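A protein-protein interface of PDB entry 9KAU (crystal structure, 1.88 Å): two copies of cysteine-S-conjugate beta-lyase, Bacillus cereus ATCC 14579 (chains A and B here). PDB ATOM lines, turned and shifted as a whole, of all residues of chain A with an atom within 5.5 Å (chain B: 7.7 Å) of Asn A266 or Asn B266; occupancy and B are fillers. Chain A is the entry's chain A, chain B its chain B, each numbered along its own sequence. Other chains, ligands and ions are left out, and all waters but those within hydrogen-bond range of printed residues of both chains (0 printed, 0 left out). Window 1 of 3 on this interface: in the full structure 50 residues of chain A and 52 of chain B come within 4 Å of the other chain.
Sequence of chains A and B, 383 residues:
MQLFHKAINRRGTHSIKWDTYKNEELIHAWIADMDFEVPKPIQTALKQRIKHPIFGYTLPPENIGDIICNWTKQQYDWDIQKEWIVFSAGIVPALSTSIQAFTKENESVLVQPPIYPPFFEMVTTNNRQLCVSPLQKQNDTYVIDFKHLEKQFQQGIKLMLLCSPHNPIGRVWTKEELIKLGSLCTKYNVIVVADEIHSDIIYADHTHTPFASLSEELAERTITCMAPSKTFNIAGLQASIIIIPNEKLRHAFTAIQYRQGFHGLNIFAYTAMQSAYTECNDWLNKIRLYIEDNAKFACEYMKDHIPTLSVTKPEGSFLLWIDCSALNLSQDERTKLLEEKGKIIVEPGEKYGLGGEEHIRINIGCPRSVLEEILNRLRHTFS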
ATOM      1  N   THR A  58     -22.846  -7.404  -2.037  1.00  0.00           N
ATOM      2  CA  THR A  58     -22.440  -8.330  -0.997  1.00  0.00           C
ATOM      3  C   THR A  58     -23.476  -9.433  -0.875  1.00  0.00           C
ATOM      4  O   THR A  58     -24.661  -9.236  -1.167  1.00  0.00           O
ATOM      5  CB  THR A  58     -22.252  -7.654   0.382  1.00  0.00           C
ATOM      6  OG1 THR A  58     -23.521  -7.295   0.936  1.00  0.00           O
ATOM      7  CG2 THR A  58     -21.368  -6.422   0.275  1.00  0.00           C
ATOM      8  N   GLY A 236     -33.672   2.097  10.929  1.00  0.00           N
ATOM      9  CA  GLY A 236     -33.199   2.828   9.771  1.00  0.00           C
ATOM     10  C   GLY A 236     -32.206   2.094   8.906  1.00  0.00           C
ATOM     11  O   GLY A 236     -31.750   2.629   7.881  1.00  0.00           O
ATOM     12  N   LEU A 237     -31.806   0.893   9.340  1.00  0.00           N
ATOM     13  CA  LEU A 237     -30.911   0.038   8.572  1.00  0.00           C
ATOM     14  C   LEU A 237     -31.649  -0.995   7.728  1.00  0.00           C
ATOM     15  O   LEU A 237     -31.042  -1.580   6.824  1.00  0.00           O
ATOM     16  CB  LEU A 237     -29.942  -0.695   9.499  1.00  0.00           C
ATOM     17  CG  LEU A 237     -29.152   0.098  10.531  1.00  0.00           C
ATOM     18  CD1 LEU A 237     -27.925  -0.715  10.961  1.00  0.00           C
ATOM     19  CD2 LEU A 237     -28.775   1.475  10.022  1.00  0.00           C
ATOM     20  N   GLN A 238     -32.934  -1.224   8.001  1.00  0.00           N
ATOM     21  CA  GLN A 238     -33.808  -2.060   7.171  1.00  0.00           C
ATOM     22  C   GLN A 238     -33.343  -3.526   7.091  1.00  0.00           C
ATOM     23  O   GLN A 238     -33.032  -4.048   6.019  1.00  0.00           O
ATOM     24  CB  GLN A 238     -33.950  -1.448   5.780  1.00  0.00           C
ATOM     25  CG  GLN A 238     -35.042  -0.418   5.697  1.00  0.00           C
ATOM     26  CD  GLN A 238     -34.659   0.743   4.818  1.00  0.00           C
ATOM     27  OE1 GLN A 238     -34.047   0.569   3.763  1.00  0.00           O
ATOM     28  NE2 GLN A 238     -35.028   1.947   5.243  1.00  0.00           N
ATOM     29  N   GLY A 264     -31.976  -8.887  -1.896  1.00  0.00           N
ATOM     30  CA  GLY A 264     -31.333  -8.884  -0.599  1.00  0.00           C
ATOM     31  C   GLY A 264     -31.157  -7.479  -0.060  1.00  0.00           C
ATOM     32  O   GLY A 264     -31.582  -6.487  -0.655  1.00  0.00           O
ATOM     33  N   LEU A 265     -30.503  -7.427   1.094  1.00  0.00           N
ATOM     34  CA  LEU A 265     -30.403  -6.244   1.940  1.00  0.00           C
ATOM     35  C   LEU A 265     -29.059  -5.541   1.769  1.00  0.00           C
ATOM     36  O   LEU A 265     -28.147  -6.027   1.098  1.00  0.00           O
ATOM     37  CB  LEU A 265     -30.606  -6.613   3.418  1.00  0.00           C
ATOM     38  CG  LEU A 265     -31.796  -7.433   3.911  1.00  0.00           C
ATOM     39  CD1 LEU A 265     -32.015  -7.174   5.390  1.00  0.00           C
ATOM     40  CD2 LEU A 265     -33.054  -7.165   3.119  1.00  0.00           C
ATOM     41  N   ASN A 266     -28.959  -4.445   2.471  1.00  0.00           N
ATOM     42  CA  ASN A 266     -27.780  -3.581   2.411  1.00  0.00           C
ATOM     43  C   ASN A 266     -26.661  -4.086   3.305  1.00  0.00           C
ATOM     44  O   ASN A 266     -26.921  -4.872   4.210  1.00  0.00           O
ATOM     45  CB  ASN A 266     -28.245  -2.155   2.719  1.00  0.00           C
ATOM     46  CG  ASN A 266     -29.089  -1.973   3.965  1.00  0.00           C
ATOM     47  OD1 ASN A 266     -30.241  -2.387   4.022  1.00  0.00           O
ATOM     48  ND2 ASN A 266     -28.537  -1.298   4.952  1.00  0.00           N
ATOM     49  N   ILE A 267     -25.480  -3.526   3.137  1.00  0.00           N
ATOM     50  CA  ILE A 267     -24.289  -4.040   3.820  1.00  0.00           C
ATOM     51  C   ILE A 267     -24.430  -4.015   5.336  1.00  0.00           C
ATOM     52  O   ILE A 267     -24.037  -4.966   6.022  1.00  0.00           O
ATOM     53  CB  ILE A 267     -23.050  -3.249   3.364  1.00  0.00           C
ATOM     54  CG1 ILE A 267     -22.669  -3.684   1.947  1.00  0.00           C
ATOM     55  CG2 ILE A 267     -21.907  -3.467   4.340  1.00  0.00           C
ATOM     56  CD1 ILE A 267     -21.714  -2.787   1.256  1.00  0.00           C
ATOM     57  N   PHE A 268     -24.929  -2.906   5.888  1.00  0.00           N
ATOM     58  CA  PHE A 268     -24.980  -2.710   7.337  1.00  0.00           C
ATOM     59  C   PHE A 268     -26.210  -3.349   7.985  1.00  0.00           C
ATOM     60  O   PHE A 268     -26.188  -3.614   9.188  1.00  0.00           O
ATOM     61  CB  PHE A 268     -24.891  -1.212   7.643  1.00  0.00           C
ATOM     62  CG  PHE A 268     -23.657  -0.539   7.049  1.00  0.00           C
ATOM     63  CD1 PHE A 268     -22.424  -0.661   7.649  1.00  0.00           C
ATOM     64  CD2 PHE A 268     -23.742   0.213   5.899  1.00  0.00           C
ATOM     65  CE1 PHE A 268     -21.312  -0.050   7.109  1.00  0.00           C
ATOM     66  CE2 PHE A 268     -22.633   0.820   5.360  1.00  0.00           C
ATOM     67  CZ  PHE A 268     -21.419   0.690   5.963  1.00  0.00           C
ATOM     68  N   ALA A 269     -27.275  -3.588   7.215  1.00  0.00           N
ATOM     69  CA  ALA A 269     -28.406  -4.372   7.704  1.00  0.00           C
ATOM     70  C   ALA A 269     -27.986  -5.799   8.027  1.00  0.00           C
ATOM     71  O   ALA A 269     -28.409  -6.365   9.039  1.00  0.00           O
ATOM     72  CB  ALA A 269     -29.530  -4.375   6.664  1.00  0.00           C
ATOM     73  N   TYR A 270     -27.176  -6.416   7.165  1.00  0.00           N
ATOM     74  CA  TYR A 270     -26.623  -7.709   7.531  1.00  0.00           C
ATOM     75  C   TYR A 270     -25.685  -7.548   8.719  1.00  0.00           C
ATOM     76  O   TYR A 270     -25.768  -8.305   9.691  1.00  0.00           O
ATOM     77  CB  TYR A 270     -25.856  -8.345   6.358  1.00  0.00           C
ATOM     78  CG  TYR A 270     -26.684  -8.826   5.179  1.00  0.00           C
ATOM     79  CD1 TYR A 270     -27.825  -9.576   5.354  1.00  0.00           C
ATOM     80  CD2 TYR A 270     -26.314  -8.514   3.894  1.00  0.00           C
ATOM     81  CE1 TYR A 270     -28.580  -9.993   4.273  1.00  0.00           C
ATOM     82  CE2 TYR A 270     -27.054  -8.916   2.822  1.00  0.00           C
ATOM     83  CZ  TYR A 270     -28.178  -9.662   3.002  1.00  0.00           C
ATOM     84  OH  TYR A 270     -28.890 -10.058   1.888  1.00  0.00           O
ATOM     85  N   THR A 271     -24.831  -6.519   8.680  1.00  0.00           N
ATOM     86  CA  THR A 271     -23.768  -6.367   9.667  1.00  0.00           C
ATOM     87  C   THR A 271     -24.326  -6.111  11.058  1.00  0.00           C
ATOM     88  O   THR A 271     -23.753  -6.564  12.055  1.00  0.00           O
ATOM     89  CB  THR A 271     -22.839  -5.238   9.238  1.00  0.00           C
ATOM     90  OG1 THR A 271     -22.514  -5.393   7.850  1.00  0.00           O
ATOM     91  CG2 THR A 271     -21.562  -5.233  10.062  1.00  0.00           C
ATOM     92  N   GLY B  56     -32.760   4.870  14.071  1.00  0.00           N
ATOM     93  CA  GLY B  56     -34.190   4.825  13.879  1.00  0.00           C
ATOM     94  C   GLY B  56     -34.583   5.286  12.491  1.00  0.00           C
ATOM     95  O   GLY B  56     -33.755   5.427  11.587  1.00  0.00           O
ATOM     96  N   THR B  58     -35.504   7.502   9.427  1.00  0.00           N
ATOM     97  CA  THR B  58     -34.828   8.685   8.948  1.00  0.00           C
ATOM     98  C   THR B  58     -35.627   9.250   7.787  1.00  0.00           C
ATOM     99  O   THR B  58     -36.365   8.520   7.123  1.00  0.00           O
ATOM    100  CB  THR B  58     -33.395   8.335   8.553  1.00  0.00           C
ATOM    101  OG1 THR B  58     -32.712   7.797   9.695  1.00  0.00           O
ATOM    102  CG2 THR B  58     -32.647   9.541   8.042  1.00  0.00           C
ATOM    103  N   LEU B  59     -35.601  10.580   7.649  1.00  0.00           N
ATOM    104  CA  LEU B  59     -36.128  11.331   6.510  1.00  0.00           C
ATOM    105  C   LEU B  59     -35.051  11.543   5.443  1.00  0.00           C
ATOM    106  O   LEU B  59     -33.847  11.433   5.716  1.00  0.00           O
ATOM    107  CB  LEU B  59     -36.677  12.695   6.971  1.00  0.00           C
ATOM    108  CG  LEU B  59     -37.876  12.874   7.929  1.00  0.00           C
ATOM    109  CD1 LEU B  59     -37.459  13.720   9.130  1.00  0.00           C
ATOM    110  CD2 LEU B  59     -39.161  13.457   7.288  1.00  0.00           C
ATOM    111  N   ALA B  89     -34.482   1.957  -4.082  1.00  0.00           N
ATOM    112  CA  ALA B  89     -33.396   1.188  -3.497  1.00  0.00           C
ATOM    113  C   ALA B  89     -32.490   0.555  -4.550  1.00  0.00           C
ATOM    114  O   ALA B  89     -31.669  -0.296  -4.211  1.00  0.00           O
ATOM    115  CB  ALA B  89     -33.977   0.102  -2.600  1.00  0.00           C
ATOM    116  N   ALA B 235     -22.639   0.246  -4.463  1.00  0.00           N
ATOM    117  CA  ALA B 235     -23.823  -0.511  -4.841  1.00  0.00           C
ATOM    118  C   ALA B 235     -24.379  -1.342  -3.685  1.00  0.00           C
ATOM    119  O   ALA B 235     -25.510  -1.826  -3.785  1.00  0.00           O
ATOM    120  CB  ALA B 235     -23.514  -1.380  -6.063  1.00  0.00           C
ATOM    121  N   GLY B 236     -23.615  -1.534  -2.604  1.00  0.00           N
ATOM    122  CA  GLY B 236     -24.168  -2.124  -1.403  1.00  0.00           C
ATOM    123  C   GLY B 236     -24.903  -1.145  -0.509  1.00  0.00           C
ATOM    124  O   GLY B 236     -25.469  -1.535   0.514  1.00  0.00           O
ATOM    125  N   LEU B 237     -24.905   0.136  -0.854  1.00  0.00           N
ATOM    126  CA  LEU B 237     -25.621   1.121  -0.060  1.00  0.00           C
ATOM    127  C   LEU B 237     -27.020   1.393  -0.579  1.00  0.00           C
ATOM    128  O   LEU B 237     -27.772   2.098   0.088  1.00  0.00           O
ATOM    129  CB  LEU B 237     -24.834   2.432   0.014  1.00  0.00           C
ATOM    130  CG  LEU B 237     -23.399   2.241   0.511  1.00  0.00           C
ATOM    131  CD1 LEU B 237     -22.827   3.528   1.042  1.00  0.00           C
ATOM    132  CD2 LEU B 237     -23.304   1.146   1.574  1.00  0.00           C
ATOM    133  N   GLN B 238     -27.355   0.925  -1.780  1.00  0.00           N
ATOM    134  CA  GLN B 238     -28.727   0.941  -2.295  1.00  0.00           C
ATOM    135  C   GLN B 238     -29.328   2.354  -2.346  1.00  0.00           C
ATOM    136  O   GLN B 238     -30.361   2.631  -1.735  1.00  0.00           O
ATOM    137  CB  GLN B 238     -29.617  -0.006  -1.498  1.00  0.00           C
ATOM    138  CG  GLN B 238     -29.312  -1.469  -1.747  1.00  0.00           C
ATOM    139  CD  GLN B 238     -29.900  -2.391  -0.694  1.00  0.00           C
ATOM    140  OE1 GLN B 238     -30.187  -1.970   0.424  1.00  0.00           O
ATOM    141  NE2 GLN B 238     -30.068  -3.658  -1.046  1.00  0.00           N
ATOM    142  N   ALA B 239     -28.677   3.242  -3.109  1.00  0.00           N
ATOM    143  CA  ALA B 239     -29.197   4.580  -3.408  1.00  0.00           C
ATOM    144  C   ALA B 239     -29.549   4.684  -4.884  1.00  0.00           C
ATOM    145  O   ALA B 239     -28.756   4.291  -5.745  1.00  0.00           O
ATOM    146  CB  ALA B 239     -28.188   5.678  -3.068  1.00  0.00           C
ATOM    147  N   PHE B 262     -42.568   0.171   0.160  1.00  0.00           N
ATOM    148  CA  PHE B 262     -41.329   0.940   0.116  1.00  0.00           C
ATOM    149  C   PHE B 262     -41.594   2.333   0.664  1.00  0.00           C
ATOM    150  O   PHE B 262     -42.547   3.002   0.251  1.00  0.00           O
ATOM    151  CB  PHE B 262     -40.808   1.033  -1.318  1.00  0.00           C
ATOM    152  CG  PHE B 262     -39.568   1.878  -1.464  1.00  0.00           C
ATOM    153  CD1 PHE B 262     -38.386   1.474  -0.905  1.00  0.00           C
ATOM    154  CD2 PHE B 262     -39.585   3.059  -2.175  1.00  0.00           C
ATOM    155  CE1 PHE B 262     -37.250   2.232  -1.036  1.00  0.00           C
ATOM    156  CE2 PHE B 262     -38.447   3.812  -2.300  1.00  0.00           C
ATOM    157  CZ  PHE B 262     -37.280   3.396  -1.728  1.00  0.00           C
ATOM    158  N   HIS B 263     -40.736   2.780   1.578  1.00  0.00           N
ATOM    159  CA  HIS B 263     -40.937   4.054   2.259  1.00  0.00           C
ATOM    160  C   HIS B 263     -39.683   4.907   2.268  1.00  0.00           C
ATOM    161  O   HIS B 263     -39.523   5.739   3.161  1.00  0.00           O
ATOM    162  CB  HIS B 263     -41.379   3.842   3.705  1.00  0.00           C
ATOM    163  CG  HIS B 263     -42.546   2.919   3.858  1.00  0.00           C
ATOM    164  ND1 HIS B 263     -43.704   3.051   3.124  1.00  0.00           N
ATOM    165  CD2 HIS B 263     -42.730   1.844   4.666  1.00  0.00           C
ATOM    166  CE1 HIS B 263     -44.553   2.099   3.470  1.00  0.00           C
ATOM    167  NE2 HIS B 263     -43.986   1.354   4.404  1.00  0.00           N
ATOM    168  N   GLY B 264     -38.783   4.706   1.329  1.00  0.00           N
ATOM    169  CA  GLY B 264     -37.549   5.455   1.292  1.00  0.00           C
ATOM    170  C   GLY B 264     -36.356   4.573   1.599  1.00  0.00           C
ATOM    171  O   GLY B 264     -36.469   3.369   1.819  1.00  0.00           O
ATOM    172  N   LEU B 265     -35.200   5.220   1.634  1.00  0.00           N
ATOM    173  CA  LEU B 265     -33.923   4.533   1.688  1.00  0.00           C
ATOM    174  C   LEU B 265     -33.382   4.487   3.108  1.00  0.00           C
ATOM    175  O   LEU B 265     -33.866   5.164   4.018  1.00  0.00           O
ATOM    176  CB  LEU B 265     -32.906   5.212   0.766  1.00  0.00           C
ATOM    177  CG  LEU B 265     -33.397   5.716  -0.582  1.00  0.00           C
ATOM    178  CD1 LEU B 265     -32.221   6.276  -1.353  1.00  0.00           C
ATOM    179  CD2 LEU B 265     -34.075   4.589  -1.328  1.00  0.00           C
ATOM    180  N   ASN B 266     -32.344   3.682   3.277  1.00  0.00           N
ATOM    181  CA  ASN B 266     -31.733   3.492   4.577  1.00  0.00           C
ATOM    182  C   ASN B 266     -30.705   4.593   4.862  1.00  0.00           C
ATOM    183  O   ASN B 266     -30.276   5.331   3.973  1.00  0.00           O
ATOM    184  CB  ASN B 266     -31.126   2.081   4.672  1.00  0.00           C
ATOM    185  CG  ASN B 266     -29.918   1.879   3.783  1.00  0.00           C
ATOM    186  OD1 ASN B 266     -28.802   2.156   4.192  1.00  0.00           O
ATOM    187  ND2 ASN B 266     -30.128   1.338   2.588  1.00  0.00           N
ATOM    188  N   ILE B 267     -30.305   4.676   6.135  1.00  0.00           N
ATOM    189  CA  ILE B 267     -29.468   5.768   6.646  1.00  0.00           C
ATOM    190  C   ILE B 267     -28.210   5.965   5.800  1.00  0.00           C
ATOM    191  O   ILE B 267     -27.797   7.100   5.534  1.00  0.00           O
ATOM    192  CB  ILE B 267     -29.124   5.503   8.125  1.00  0.00           C
ATOM    193  CG1 ILE B 267     -30.270   5.958   9.021  1.00  0.00           C
ATOM    194  CG2 ILE B 267     -27.859   6.197   8.516  1.00  0.00           C
ATOM    195  CD1 ILE B 267     -30.179   5.431  10.429  1.00  0.00           C
ATOM    196  N   PHE B 268     -27.568   4.875   5.388  1.00  0.00           N
ATOM    197  CA  PHE B 268     -26.292   4.989   4.678  1.00  0.00           C
ATOM    198  C   PHE B 268     -26.471   5.307   3.199  1.00  0.00           C
ATOM    199  O   PHE B 268     -25.574   5.890   2.585  1.00  0.00           O
ATOM    200  CB  PHE B 268     -25.493   3.701   4.848  1.00  0.00           C
ATOM    201  CG  PHE B 268     -25.280   3.331   6.279  1.00  0.00           C
ATOM    202  CD1 PHE B 268     -24.199   3.825   6.972  1.00  0.00           C
ATOM    203  CD2 PHE B 268     -26.186   2.530   6.939  1.00  0.00           C
ATOM    204  CE1 PHE B 268     -24.003   3.509   8.290  1.00  0.00           C
ATOM    205  CE2 PHE B 268     -25.993   2.216   8.256  1.00  0.00           C
ATOM    206  CZ  PHE B 268     -24.900   2.707   8.934  1.00  0.00           C
ATOM    207  N   ALA B 269     -27.618   4.949   2.621  1.00  0.00           N
ATOM    208  CA  ALA B 269     -27.937   5.389   1.269  1.00  0.00           C
ATOM    209  C   ALA B 269     -28.120   6.899   1.206  1.00  0.00           C
ATOM    210  O   ALA B 269     -27.599   7.556   0.301  1.00  0.00           O
ATOM    211  CB  ALA B 269     -29.195   4.680   0.770  1.00  0.00           C
ATOM    212  N   TYR B 270     -28.836   7.480   2.172  1.00  0.00           N
ATOM    213  CA  TYR B 270     -28.976   8.932   2.175  1.00  0.00           C
ATOM    214  C   TYR B 270     -27.624   9.595   2.389  1.00  0.00           C
ATOM    215  O   TYR B 270     -27.271  10.547   1.680  1.00  0.00           O
ATOM    216  CB  TYR B 270     -29.978   9.382   3.245  1.00  0.00           C
ATOM    217  CG  TYR B 270     -31.423   9.130   2.880  1.00  0.00           C
ATOM    218  CD1 TYR B 270     -31.981   9.695   1.764  1.00  0.00           C
ATOM    219  CD2 TYR B 270     -32.215   8.300   3.650  1.00  0.00           C
ATOM    220  CE1 TYR B 270     -33.286   9.453   1.416  1.00  0.00           C
ATOM    221  CE2 TYR B 270     -33.532   8.058   3.307  1.00  0.00           C
ATOM    222  CZ  TYR B 270     -34.062   8.637   2.185  1.00  0.00           C
ATOM    223  OH  TYR B 270     -35.370   8.406   1.829  1.00  0.00           O
ATOM    224  N   THR B 271     -26.834   9.083   3.335  1.00  0.00           N
ATOM    225  CA  THR B 271     -25.584   9.760   3.666  1.00  0.00           C
ATOM    226  C   THR B 271     -24.584   9.691   2.521  1.00  0.00           C
ATOM    227  O   THR B 271     -23.949  10.695   2.193  1.00  0.00           O
ATOM    228  CB  THR B 271     -24.969   9.156   4.928  1.00  0.00           C
ATOM    229  OG1 THR B 271     -26.005   8.795   5.849  1.00  0.00           O
ATOM    230  CG2 THR B 271     -24.011  10.150   5.590  1.00  0.00           C
ATOM    231  N   ALA B 272     -24.462   8.532   1.870  1.00  0.00           N
ATOM    232  CA  ALA B 272     -23.468   8.382   0.808  1.00  0.00           C
ATOM    233  C   ALA B 272     -23.852   9.172  -0.435  1.00  0.00           C
ATOM    234  O   ALA B 272     -23.033   9.915  -0.981  1.00  0.00           O
ATOM    235  CB  ALA B 272     -23.287   6.904   0.463  1.00  0.00           C
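N of Gly A236 lies close to O of Gly B56 (3.4 Å).
The backbone carbonyl oxygen (O) of Gly A236 lies within hydrogen-bond range of the backbone NH (N) of Ile B267 (3.1 Å).
The side-chain amide nitrogen (NE2) of Gln B238 sits at hydrogen-bond distance from the backbone carbonyl oxygen (O) of Gly A264, 3.2 Å away.
The backbone NH (N) of Asn A266 lies close to the side-chain amide oxygen (OE1) of Gln B238.
N of Ile A267 lies within hydrogen-bond range of O of Gly B236 (3.3 Å).
The backbone carbonyl oxygen (O) of Leu A237 sits close to the side-chain amide oxygen (OD1) of Asn A266, at 3.0 Å.
The backbone NH (N) of Leu A265 sits at hydrogen-bond distance from the side-chain hydroxyl (OH) of Tyr A270 (3.2 Å).
The side-chain hydroxyl of Thr A271 sits at hydrogen-bond distance from the backbone carbonyl oxygen of Ile A267 (2.4 Å).
The backbone carbonyl oxygen (O) of Gly B56 is in hydrogen-bond range of the side-chain hydroxyl (OG1) of Thr B58 (3.2 Å).
OH of Tyr B270 is in hydrogen-bond range of N of Leu B265, 3.2 Å away.
OG1 of Thr B271 sits at hydrogen-bond distance from O of Ile B267, at 2.5 Å.
O of Gly A236 touches CB of Asn B266, at 3.3 Å.
CE2 of Phe B268 touches CD2 of Leu A237 (3.4 Å).
Gln A238 touches Gly B264.
O of Leu B265 touches NE2 of Gln A238, at 3.6 Å.
Gln A238 touches Asn B266 (OE1 to CB, 3.4 Å).
Leu A265 touches Gln B238.
Gly B236 touches Asn A266 (O to CB, 3.6 Å).
Asn B266 touches Asn A266.
Phe A268 touches Leu B237.
Phe A268 touches Phe B268.
Printed residues of chain B within 4 Å of Gly A236: Gly B56 (3.2 Å), Asn B266 (3.3 Å) and Ile B267 (3.1 Å).
Of the printed residues of chain B, Ile A267 touches Gly B236 (3.3 Å).
Of chain A, only Gly A236, Gln A238 and Asn A266 come within 4 Å of Asn B266.
The nearest residue of chain A that does not touch Asn B266 is Leu A237 (4.2 Å).
The nearest printed residue of chain B that does not touch Gly A236 is Thr B58 (5.0 Å).
Hydrophobic or aromatic side chains of chain A within 4 Å of the printed part of chain B: Leu A237, Ile A267 and Phe A268.
Among the printed residues, 15 pairs touch across the chains.
Among the printed residues, no Asp or Glu carboxylate lies within 4 Å of a Lys or Arg side-chain nitrogen of the other chain.
Gly A236 touches Asn B266, and with the chains exchanged Asn A266 touches Gly B236.
Gly A236 touches Ile B267, and with the chains exchanged Ile A267 touches Gly B236.
Leu A237 touches Phe B268, and with the chains exchanged Phe A268 touches Leu B237.
Gln A238 touches Gly B264, and with the chains exchanged Gly A264 touches Gln B238.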
